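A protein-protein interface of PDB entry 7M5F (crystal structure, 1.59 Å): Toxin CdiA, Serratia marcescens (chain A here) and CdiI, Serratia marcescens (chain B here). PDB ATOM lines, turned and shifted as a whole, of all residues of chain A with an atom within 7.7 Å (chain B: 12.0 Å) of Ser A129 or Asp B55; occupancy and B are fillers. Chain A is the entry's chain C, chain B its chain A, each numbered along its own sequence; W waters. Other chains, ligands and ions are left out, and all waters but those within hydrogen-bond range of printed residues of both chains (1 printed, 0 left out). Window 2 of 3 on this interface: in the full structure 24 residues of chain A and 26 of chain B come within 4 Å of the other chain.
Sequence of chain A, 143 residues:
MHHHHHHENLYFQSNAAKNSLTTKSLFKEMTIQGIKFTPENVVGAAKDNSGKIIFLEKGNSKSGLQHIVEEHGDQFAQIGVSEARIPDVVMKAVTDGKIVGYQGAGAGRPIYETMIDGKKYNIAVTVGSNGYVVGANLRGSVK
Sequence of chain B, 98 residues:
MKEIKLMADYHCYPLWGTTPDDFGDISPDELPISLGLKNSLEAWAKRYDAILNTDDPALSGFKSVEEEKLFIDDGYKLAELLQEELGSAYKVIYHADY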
ATOM      1  N   GLN A  33       7.597  22.731  24.241  1.00  0.00           N
ATOM      2  CA  GLN A  33       8.780  22.549  23.418  1.00  0.00           C
ATOM      3  C   GLN A  33       9.524  23.852  23.192  1.00  0.00           C
ATOM      4  O   GLN A  33      10.595  23.840  22.569  1.00  0.00           O
ATOM      5  CB  GLN A  33       8.425  21.860  22.101  1.00  0.00           C
ATOM      6  CG  GLN A  33       7.987  22.727  21.007  1.00  0.00           C
ATOM      7  CD  GLN A  33       7.661  21.920  19.739  1.00  0.00           C
ATOM      8  OE1 GLN A  33       8.441  21.880  18.791  1.00  0.00           O
ATOM      9  NE2 GLN A  33       6.523  21.277  19.744  1.00  0.00           N
ATOM     10  N   ILE A  35       8.239  26.875  21.839  1.00  0.00           N
ATOM     11  CA  ILE A  35       7.751  27.789  20.814  1.00  0.00           C
ATOM     12  C   ILE A  35       7.035  28.950  21.491  1.00  0.00           C
ATOM     13  O   ILE A  35       6.209  28.741  22.387  1.00  0.00           O
ATOM     14  CB  ILE A  35       6.829  27.064  19.826  1.00  0.00           C
ATOM     15  CG1 ILE A  35       7.585  25.958  19.096  1.00  0.00           C
ATOM     16  CG2 ILE A  35       6.228  28.051  18.818  1.00  0.00           C
ATOM     17  CD1 ILE A  35       6.668  24.968  18.457  1.00  0.00           C
ATOM     18  N   LYS A  52       5.902  15.326  14.215  1.00  0.00           N
ATOM     19  CA  LYS A  52       6.365  16.711  14.281  1.00  0.00           C
ATOM     20  C   LYS A  52       5.168  17.644  14.215  1.00  0.00           C
ATOM     21  O   LYS A  52       4.347  17.534  13.293  1.00  0.00           O
ATOM     22  CB  LYS A  52       7.310  17.030  13.119  1.00  0.00           C
ATOM     23  CG  LYS A  52       7.889  18.442  13.175  1.00  0.00           C
ATOM     24  CD  LYS A  52       8.896  18.730  12.049  1.00  0.00           C
ATOM     25  CE  LYS A  52       9.440  20.188  12.129  1.00  0.00           C
ATOM     26  NZ  LYS A  52      10.435  20.608  11.046  1.00  0.00           N
ATOM     27  N   ILE A  53       5.086  18.567  15.172  1.00  0.00           N
ATOM     28  CA  ILE A  53       4.091  19.629  15.140  1.00  0.00           C
ATOM     29  C   ILE A  53       4.473  20.642  14.065  1.00  0.00           C
ATOM     30  O   ILE A  53       5.580  21.189  14.067  1.00  0.00           O
ATOM     31  CB  ILE A  53       3.929  20.308  16.502  1.00  0.00           C
ATOM     32  CG1 ILE A  53       3.385  19.301  17.506  1.00  0.00           C
ATOM     33  CG2 ILE A  53       2.967  21.506  16.362  1.00  0.00           C
ATOM     34  CD1 ILE A  53       3.123  19.888  18.897  1.00  0.00           C
ATOM     35  N   ILE A  54       3.540  20.881  13.147  1.00  0.00           N
ATOM     36  CA  ILE A  54       3.660  21.870  12.086  1.00  0.00           C
ATOM     37  C   ILE A  54       2.591  22.933  12.322  1.00  0.00           C
ATOM     38  O   ILE A  54       1.456  22.611  12.672  1.00  0.00           O
ATOM     39  CB  ILE A  54       3.466  21.205  10.708  1.00  0.00           C
ATOM     40  CG1 ILE A  54       4.406  20.014  10.499  1.00  0.00           C
ATOM     41  CG2 ILE A  54       3.645  22.210   9.571  1.00  0.00           C
ATOM     42  CD1 ILE A  54       5.815  20.328  10.543  1.00  0.00           C
ATOM     43  N   PHE A  55       2.954  24.196  12.184  1.00  0.00           N
ATOM     44  CA  PHE A  55       1.967  25.233  12.440  1.00  0.00           C
ATOM     45  C   PHE A  55       2.194  26.401  11.504  1.00  0.00           C
ATOM     46  O   PHE A  55       3.314  26.652  11.025  1.00  0.00           O
ATOM     47  CB  PHE A  55       1.975  25.670  13.926  1.00  0.00           C
ATOM     48  CG  PHE A  55       3.220  26.359  14.355  1.00  0.00           C
ATOM     49  CD1 PHE A  55       4.367  25.636  14.636  1.00  0.00           C
ATOM     50  CD2 PHE A  55       3.252  27.739  14.496  1.00  0.00           C
ATOM     51  CE1 PHE A  55       5.507  26.257  15.018  1.00  0.00           C
ATOM     52  CE2 PHE A  55       4.422  28.372  14.884  1.00  0.00           C
ATOM     53  CZ  PHE A  55       5.544  27.620  15.164  1.00  0.00           C
ATOM     54  N   VAL A 127       9.370  24.505   5.783  1.00  0.00           N
ATOM     55  CA  VAL A 127       9.055  24.533   7.213  1.00  0.00           C
ATOM     56  C   VAL A 127      10.353  24.748   7.976  1.00  0.00           C
ATOM     57  O   VAL A 127      11.385  24.148   7.650  1.00  0.00           O
ATOM     58  CB  VAL A 127       8.378  23.228   7.664  1.00  0.00           C
ATOM     59  CG1 VAL A 127       8.062  23.251   9.144  1.00  0.00           C
ATOM     60  CG2 VAL A 127       7.113  23.002   6.897  1.00  0.00           C
ATOM     61  N   GLY A 128      10.295  25.581   9.019  1.00  0.00           N
ATOM     62  CA  GLY A 128      11.423  25.747   9.901  1.00  0.00           C
ATOM     63  C   GLY A 128      11.649  24.544  10.791  1.00  0.00           C
ATOM     64  O   GLY A 128      10.815  23.656  10.924  1.00  0.00           O
ATOM     65  N   SER A 129      12.812  24.530  11.441  1.00  0.00           N
ATOM     66  CA  SER A 129      13.109  23.414  12.332  1.00  0.00           C
ATOM     67  C   SER A 129      12.148  23.371  13.515  1.00  0.00           C
ATOM     68  O   SER A 129      11.997  22.306  14.131  1.00  0.00           O
ATOM     69  CB  SER A 129      14.542  23.503  12.817  1.00  0.00           C
ATOM     70  OG  SER A 129      14.740  24.627  13.636  1.00  0.00           O
ATOM     71  N   ASN A 130      11.490  24.480  13.829  1.00  0.00           N
ATOM     72  CA  ASN A 130      10.522  24.534  14.923  1.00  0.00           C
ATOM     73  C   ASN A 130       9.109  24.200  14.483  1.00  0.00           C
ATOM     74  O   ASN A 130       8.203  24.242  15.315  1.00  0.00           O
ATOM     75  CB  ASN A 130      10.546  25.922  15.580  1.00  0.00           C
ATOM     76  CG  ASN A 130      10.093  27.015  14.640  1.00  0.00           C
ATOM     77  OD1 ASN A 130      10.059  26.838  13.432  1.00  0.00           O
ATOM     78  ND2 ASN A 130       9.790  28.173  15.193  1.00  0.00           N
ATOM     79  N   GLY A 131       8.908  23.853  13.213  1.00  0.00           N
ATOM     80  CA  GLY A 131       7.592  23.524  12.691  1.00  0.00           C
ATOM     81  C   GLY A 131       6.844  24.659  12.023  1.00  0.00           C
ATOM     82  O   GLY A 131       5.767  24.430  11.468  1.00  0.00           O
ATOM     83  N   TYR A 132       7.388  25.873  12.053  1.00  0.00           N
ATOM     84  CA  TYR A 132       6.738  27.039  11.477  1.00  0.00           C
ATOM     85  C   TYR A 132       6.741  26.967   9.960  1.00  0.00           C
ATOM     86  O   TYR A 132       7.794  26.865   9.328  1.00  0.00           O
ATOM     87  CB  TYR A 132       7.491  28.283  11.965  1.00  0.00           C
ATOM     88  CG  TYR A 132       7.027  29.656  11.508  1.00  0.00           C
ATOM     89  CD1 TYR A 132       7.305  30.119  10.225  1.00  0.00           C
ATOM     90  CD2 TYR A 132       6.344  30.491  12.361  1.00  0.00           C
ATOM     91  CE1 TYR A 132       6.905  31.354   9.818  1.00  0.00           C
ATOM     92  CE2 TYR A 132       5.964  31.764  11.957  1.00  0.00           C
ATOM     93  CZ  TYR A 132       6.256  32.183  10.692  1.00  0.00           C
ATOM     94  OH  TYR A 132       5.863  33.440  10.306  1.00  0.00           O
ATOM     95  N   VAL A 134       6.945  28.343   6.475  1.00  0.00           N
ATOM     96  CA  VAL A 134       7.611  29.546   5.971  1.00  0.00           C
ATOM     97  C   VAL A 134       6.994  30.010   4.660  1.00  0.00           C
ATOM     98  O   VAL A 134       6.658  31.182   4.506  1.00  0.00           O
ATOM     99  CB  VAL A 134       9.114  29.292   5.788  1.00  0.00           C
ATOM    100  CG1 VAL A 134       9.811  30.543   5.298  1.00  0.00           C
ATOM    101  CG2 VAL A 134       9.786  28.812   7.049  1.00  0.00           C
ATOM    102  N   TYR B  10      12.149  31.063  -0.712  1.00  0.00           N
ATOM    103  CA  TYR B  10      13.140  30.269  -0.006  1.00  0.00           C
ATOM    104  C   TYR B  10      13.248  28.855  -0.564  1.00  0.00           C
ATOM    105  O   TYR B  10      12.267  28.118  -0.617  1.00  0.00           O
ATOM    106  CB  TYR B  10      12.779  30.201   1.463  1.00  0.00           C
ATOM    107  CG  TYR B  10      12.571  31.539   2.117  1.00  0.00           C
ATOM    108  CD1 TYR B  10      13.639  32.376   2.384  1.00  0.00           C
ATOM    109  CD2 TYR B  10      11.308  31.962   2.485  1.00  0.00           C
ATOM    110  CE1 TYR B  10      13.465  33.579   3.015  1.00  0.00           C
ATOM    111  CE2 TYR B  10      11.118  33.179   3.113  1.00  0.00           C
ATOM    112  CZ  TYR B  10      12.203  33.986   3.378  1.00  0.00           C
ATOM    113  OH  TYR B  10      12.068  35.190   4.017  1.00  0.00           O
ATOM    114  N   HIS B  11      14.481  28.447  -0.870  1.00  0.00           N
ATOM    115  CA  HIS B  11      14.803  27.082  -1.298  1.00  0.00           C
ATOM    116  C   HIS B  11      14.133  26.716  -2.609  1.00  0.00           C
ATOM    117  O   HIS B  11      13.869  25.540  -2.858  1.00  0.00           O
ATOM    118  CB  HIS B  11      14.467  26.075  -0.213  1.00  0.00           C
ATOM    119  CG  HIS B  11      15.169  26.341   1.080  1.00  0.00           C
ATOM    120  ND1 HIS B  11      16.521  26.582   1.147  1.00  0.00           N
ATOM    121  CD2 HIS B  11      14.702  26.424   2.347  1.00  0.00           C
ATOM    122  CE1 HIS B  11      16.863  26.789   2.413  1.00  0.00           C
ATOM    123  NE2 HIS B  11      15.780  26.692   3.160  1.00  0.00           N
ATOM    124  N   ASP B  49      17.759  33.453   0.118  1.00  0.00           N
ATOM    125  CA  ASP B  49      17.827  32.318   1.028  1.00  0.00           C
ATOM    126  C   ASP B  49      18.554  32.692   2.312  1.00  0.00           C
ATOM    127  O   ASP B  49      18.245  32.158   3.384  1.00  0.00           O
ATOM    128  CB  ASP B  49      18.532  31.136   0.359  1.00  0.00           C
ATOM    129  CG  ASP B  49      17.674  30.426  -0.665  1.00  0.00           C
ATOM    130  OD1 ASP B  49      16.442  30.563  -0.655  1.00  0.00           O
ATOM    131  OD2 ASP B  49      18.265  29.704  -1.510  1.00  0.00           O
ATOM    132  N   ALA B  50      19.532  33.603   2.224  1.00  0.00           N
ATOM    133  CA  ALA B  50      20.338  33.965   3.376  1.00  0.00           C
ATOM    134  C   ALA B  50      19.568  34.746   4.434  1.00  0.00           C
ATOM    135  O   ALA B  50      20.055  34.858   5.563  1.00  0.00           O
ATOM    136  CB  ALA B  50      21.554  34.792   2.948  1.00  0.00           C
ATOM    137  N   ILE B  51      18.401  35.304   4.098  1.00  0.00           N
ATOM    138  CA  ILE B  51      17.654  36.057   5.092  1.00  0.00           C
ATOM    139  C   ILE B  51      16.793  35.142   5.960  1.00  0.00           C
ATOM    140  O   ILE B  51      16.317  35.570   7.015  1.00  0.00           O
ATOM    141  CB  ILE B  51      16.773  37.185   4.518  1.00  0.00           C
ATOM    142  CG1 ILE B  51      15.485  36.665   3.886  1.00  0.00           C
ATOM    143  CG2 ILE B  51      17.544  38.044   3.551  1.00  0.00           C
ATOM    144  CD1 ILE B  51      14.498  37.783   3.522  1.00  0.00           C
ATOM    145  N   LEU B  52      16.668  33.866   5.590  1.00  0.00           N
ATOM    146  CA  LEU B  52      15.833  32.931   6.338  1.00  0.00           C
ATOM    147  C   LEU B  52      16.500  32.555   7.654  1.00  0.00           C
ATOM    148  O   LEU B  52      17.661  32.139   7.683  1.00  0.00           O
ATOM    149  CB  LEU B  52      15.574  31.678   5.496  1.00  0.00           C
ATOM    150  CG  LEU B  52      14.753  30.579   6.157  1.00  0.00           C
ATOM    151  CD1 LEU B  52      13.368  31.076   6.471  1.00  0.00           C
ATOM    152  CD2 LEU B  52      14.685  29.343   5.270  1.00  0.00           C
ATOM    153  N   ASN B  53      15.769  32.710   8.754  1.00  0.00           N
ATOM    154  CA  ASN B  53      16.176  32.185  10.055  1.00  0.00           C
ATOM    155  C   ASN B  53      15.514  30.821  10.195  1.00  0.00           C
ATOM    156  O   ASN B  53      14.321  30.736  10.444  1.00  0.00           O
ATOM    157  CB  ASN B  53      15.747  33.150  11.147  1.00  0.00           C
ATOM    158  CG  ASN B  53      16.213  32.720  12.525  1.00  0.00           C
ATOM    159  OD1 ASN B  53      16.320  31.529  12.821  1.00  0.00           O
ATOM    160  ND2 ASN B  53      16.540  33.693  13.352  1.00  0.00           N
ATOM    161  N   THR B  54      16.285  29.739  10.000  1.00  0.00           N
ATOM    162  CA  THR B  54      15.666  28.419   9.845  1.00  0.00           C
ATOM    163  C   THR B  54      15.128  27.898  11.164  1.00  0.00           C
ATOM    164  O   THR B  54      14.166  27.115  11.179  1.00  0.00           O
ATOM    165  CB  THR B  54      16.669  27.424   9.261  1.00  0.00           C
ATOM    166  OG1 THR B  54      16.915  27.742   7.883  1.00  0.00           O
ATOM    167  CG2 THR B  54      16.136  26.002   9.360  1.00  0.00           C
ATOM    168  N   ASP B  55      15.735  28.307  12.279  1.00  0.00           N
ATOM    169  CA  ASP B  55      15.271  27.885  13.586  1.00  0.00           C
ATOM    170  C   ASP B  55      14.125  28.733  14.122  1.00  0.00           C
ATOM    171  O   ASP B  55      13.423  28.294  15.032  1.00  0.00           O
ATOM    172  CB  ASP B  55      16.433  27.925  14.585  1.00  0.00           C
ATOM    173  CG  ASP B  55      17.512  26.901  14.277  1.00  0.00           C
ATOM    174  OD1 ASP B  55      17.253  25.940  13.513  1.00  0.00           O
ATOM    175  OD2 ASP B  55      18.627  27.050  14.815  1.00  0.00           O
ATOM    176  N   ASP B  56      13.929  29.939  13.598  1.00  0.00           N
ATOM    177  CA  ASP B  56      12.880  30.846  14.078  1.00  0.00           C
ATOM    178  C   ASP B  56      12.482  31.735  12.914  1.00  0.00           C
ATOM    179  O   ASP B  56      12.844  32.912  12.849  1.00  0.00           O
ATOM    180  CB  ASP B  56      13.392  31.658  15.265  1.00  0.00           C
ATOM    181  CG  ASP B  56      12.308  32.411  15.987  1.00  0.00           C
ATOM    182  OD1 ASP B  56      11.161  32.483  15.496  1.00  0.00           O
ATOM    183  OD2 ASP B  56      12.629  32.949  17.070  1.00  0.00           O
ATOM    184  N   PRO B  57      11.757  31.180  11.939  1.00  0.00           N
ATOM    185  CA  PRO B  57      11.596  31.896  10.667  1.00  0.00           C
ATOM    186  C   PRO B  57      10.811  33.183  10.775  1.00  0.00           C
ATOM    187  O   PRO B  57      10.948  34.026   9.881  1.00  0.00           O
ATOM    188  CB  PRO B  57      10.889  30.876   9.768  1.00  0.00           C
ATOM    189  CG  PRO B  57      11.190  29.559  10.407  1.00  0.00           C
ATOM    190  CD  PRO B  57      11.238  29.804  11.870  1.00  0.00           C
ATOM    191  N   ALA B  58      10.025  33.382  11.838  1.00  0.00           N
ATOM    192  CA  ALA B  58       9.344  34.654  12.016  1.00  0.00           C
ATOM    193  C   ALA B  58      10.312  35.825  12.127  1.00  0.00           C
ATOM    194  O   ALA B  58       9.904  36.971  11.910  1.00  0.00           O
ATOM    195  CB  ALA B  58       8.461  34.613  13.261  1.00  0.00           C
ATOM    196  N   LEU B  59      11.577  35.563  12.441  1.00  0.00           N
ATOM    197  CA  LEU B  59      12.595  36.591  12.558  1.00  0.00           C
ATOM    198  C   LEU B  59      13.353  36.853  11.262  1.00  0.00           C
ATOM    199  O   LEU B  59      14.316  37.629  11.276  1.00  0.00           O
ATOM    200  CB  LEU B  59      13.603  36.204  13.630  1.00  0.00           C
ATOM    201  CG  LEU B  59      13.076  36.008  15.039  1.00  0.00           C
ATOM    202  CD1 LEU B  59      14.234  35.804  16.010  1.00  0.00           C
ATOM    203  CD2 LEU B  59      12.231  37.198  15.438  1.00  0.00           C
ATOM    204  N   SER B  60      12.967  36.223  10.167  1.00  0.00           N
ATOM    205  CA  SER B  60      13.695  36.379   8.917  1.00  0.00           C
ATOM    206  C   SER B  60      13.655  37.819   8.424  1.00  0.00           C
ATOM    207  O   SER B  60      12.647  38.518   8.567  1.00  0.00           O
ATOM    208  CB  SER B  60      13.093  35.463   7.873  1.00  0.00           C
ATOM    209  OG  SER B  60      13.167  34.101   8.276  1.00  0.00           O
ATOM    210  N   GLY B  61      14.749  38.249   7.809  1.00  0.00           N
ATOM    211  CA  GLY B  61      14.798  39.571   7.224  1.00  0.00           C
ATOM    212  C   GLY B  61      16.207  39.940   6.841  1.00  0.00           C
ATOM    213  O   GLY B  61      17.168  39.269   7.187  1.00  0.00           O
HETATM  214  O   HOH W   1       9.175  31.205  13.944  1.00  0.00           O
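Of the 15 printed residues of chain B, 5 touch a printed residue of chain A.
Printed residues of chain B that touch a printed residue of chain A: Tyr B10, Leu B52, Thr B54, Asp B55 and Pro B57.
Hydrophobic or aromatic side chains of chain B within 4 Å of the printed part of chain A: Tyr B10, Leu B52 and Pro B57.
Hydrophobic or aromatic side chains of chain A within 4 Å of the printed part of chain B: Tyr A132 and Val A134.
Along chain A the printed residues that touch a printed residue of chain B span positions 128 to 134.
Among the printed residues, 10 pairs touch across the chains.
Among the printed residues, no Asp or Glu carboxylate lies within 4 Å of a Lys or Arg side-chain nitrogen of the other chain.
Ile A35 touches none of the printed residues of chain B.
No residue of chain B comes within 4 Å of Val A127.
Printed residues of chain B within 4 Å of Gly A128: Thr B54 and Pro B57.
Of chain B, only Thr B54 (2.9 Å) and Asp B55 (2.8 Å) come within 4 Å of Ser A129.
Asn A130 touches two residues of chain B.
No residue of chain B comes within 4 Å of Gly A131.
Printed residues of chain B within 4 Å of Tyr A132: Pro B57 (3.7 Å).
Printed residues of chain A within 4 Å of Tyr B10: Val A134 (3.5 Å).
Asp B55 touches just these residues of chain A: Ser A129 (2.8 Å) and Asn A130 (3.6 Å).
Water W1 lies within hydrogen-bond range of OD1 of Asp B56 (2.8 Å), N of Ala B58 (3.1 Å) and ND2 of Asn A130 (3.3 Å).
The side-chain amide oxygen (OD1) of Asn B53 lies close to the backbone NH (N) of Asp B55, 3.3 Å away.
O of Pro B57 sits at hydrogen-bond distance from OG of Ser B60 (2.7 Å).
O of Gly A128 is in hydrogen-bond range of NZ of Lys A52, 3.1 Å away.
OD1 of Asn A130 lies within hydrogen-bond range of N of Tyr A132 (3.2 Å).
Among the printed residues, merely in contact across the chains: Gly A128 with Thr B54, Val A134 with Tyr B10, Asn A130 with Pro B57, Val A134 with Pro B57, Asn A130 with Asp B55, Tyr A132 with Pro B57, Val A134 with Leu B52 and Gly A128 with Pro B57.
The backbone carbonyl oxygen of Thr B54 sits at hydrogen-bond distance from the backbone NH of Ser A129 (2.9 Å).
OG of Ser A129 sits at hydrogen-bond distance from OD1 of Asp B55.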
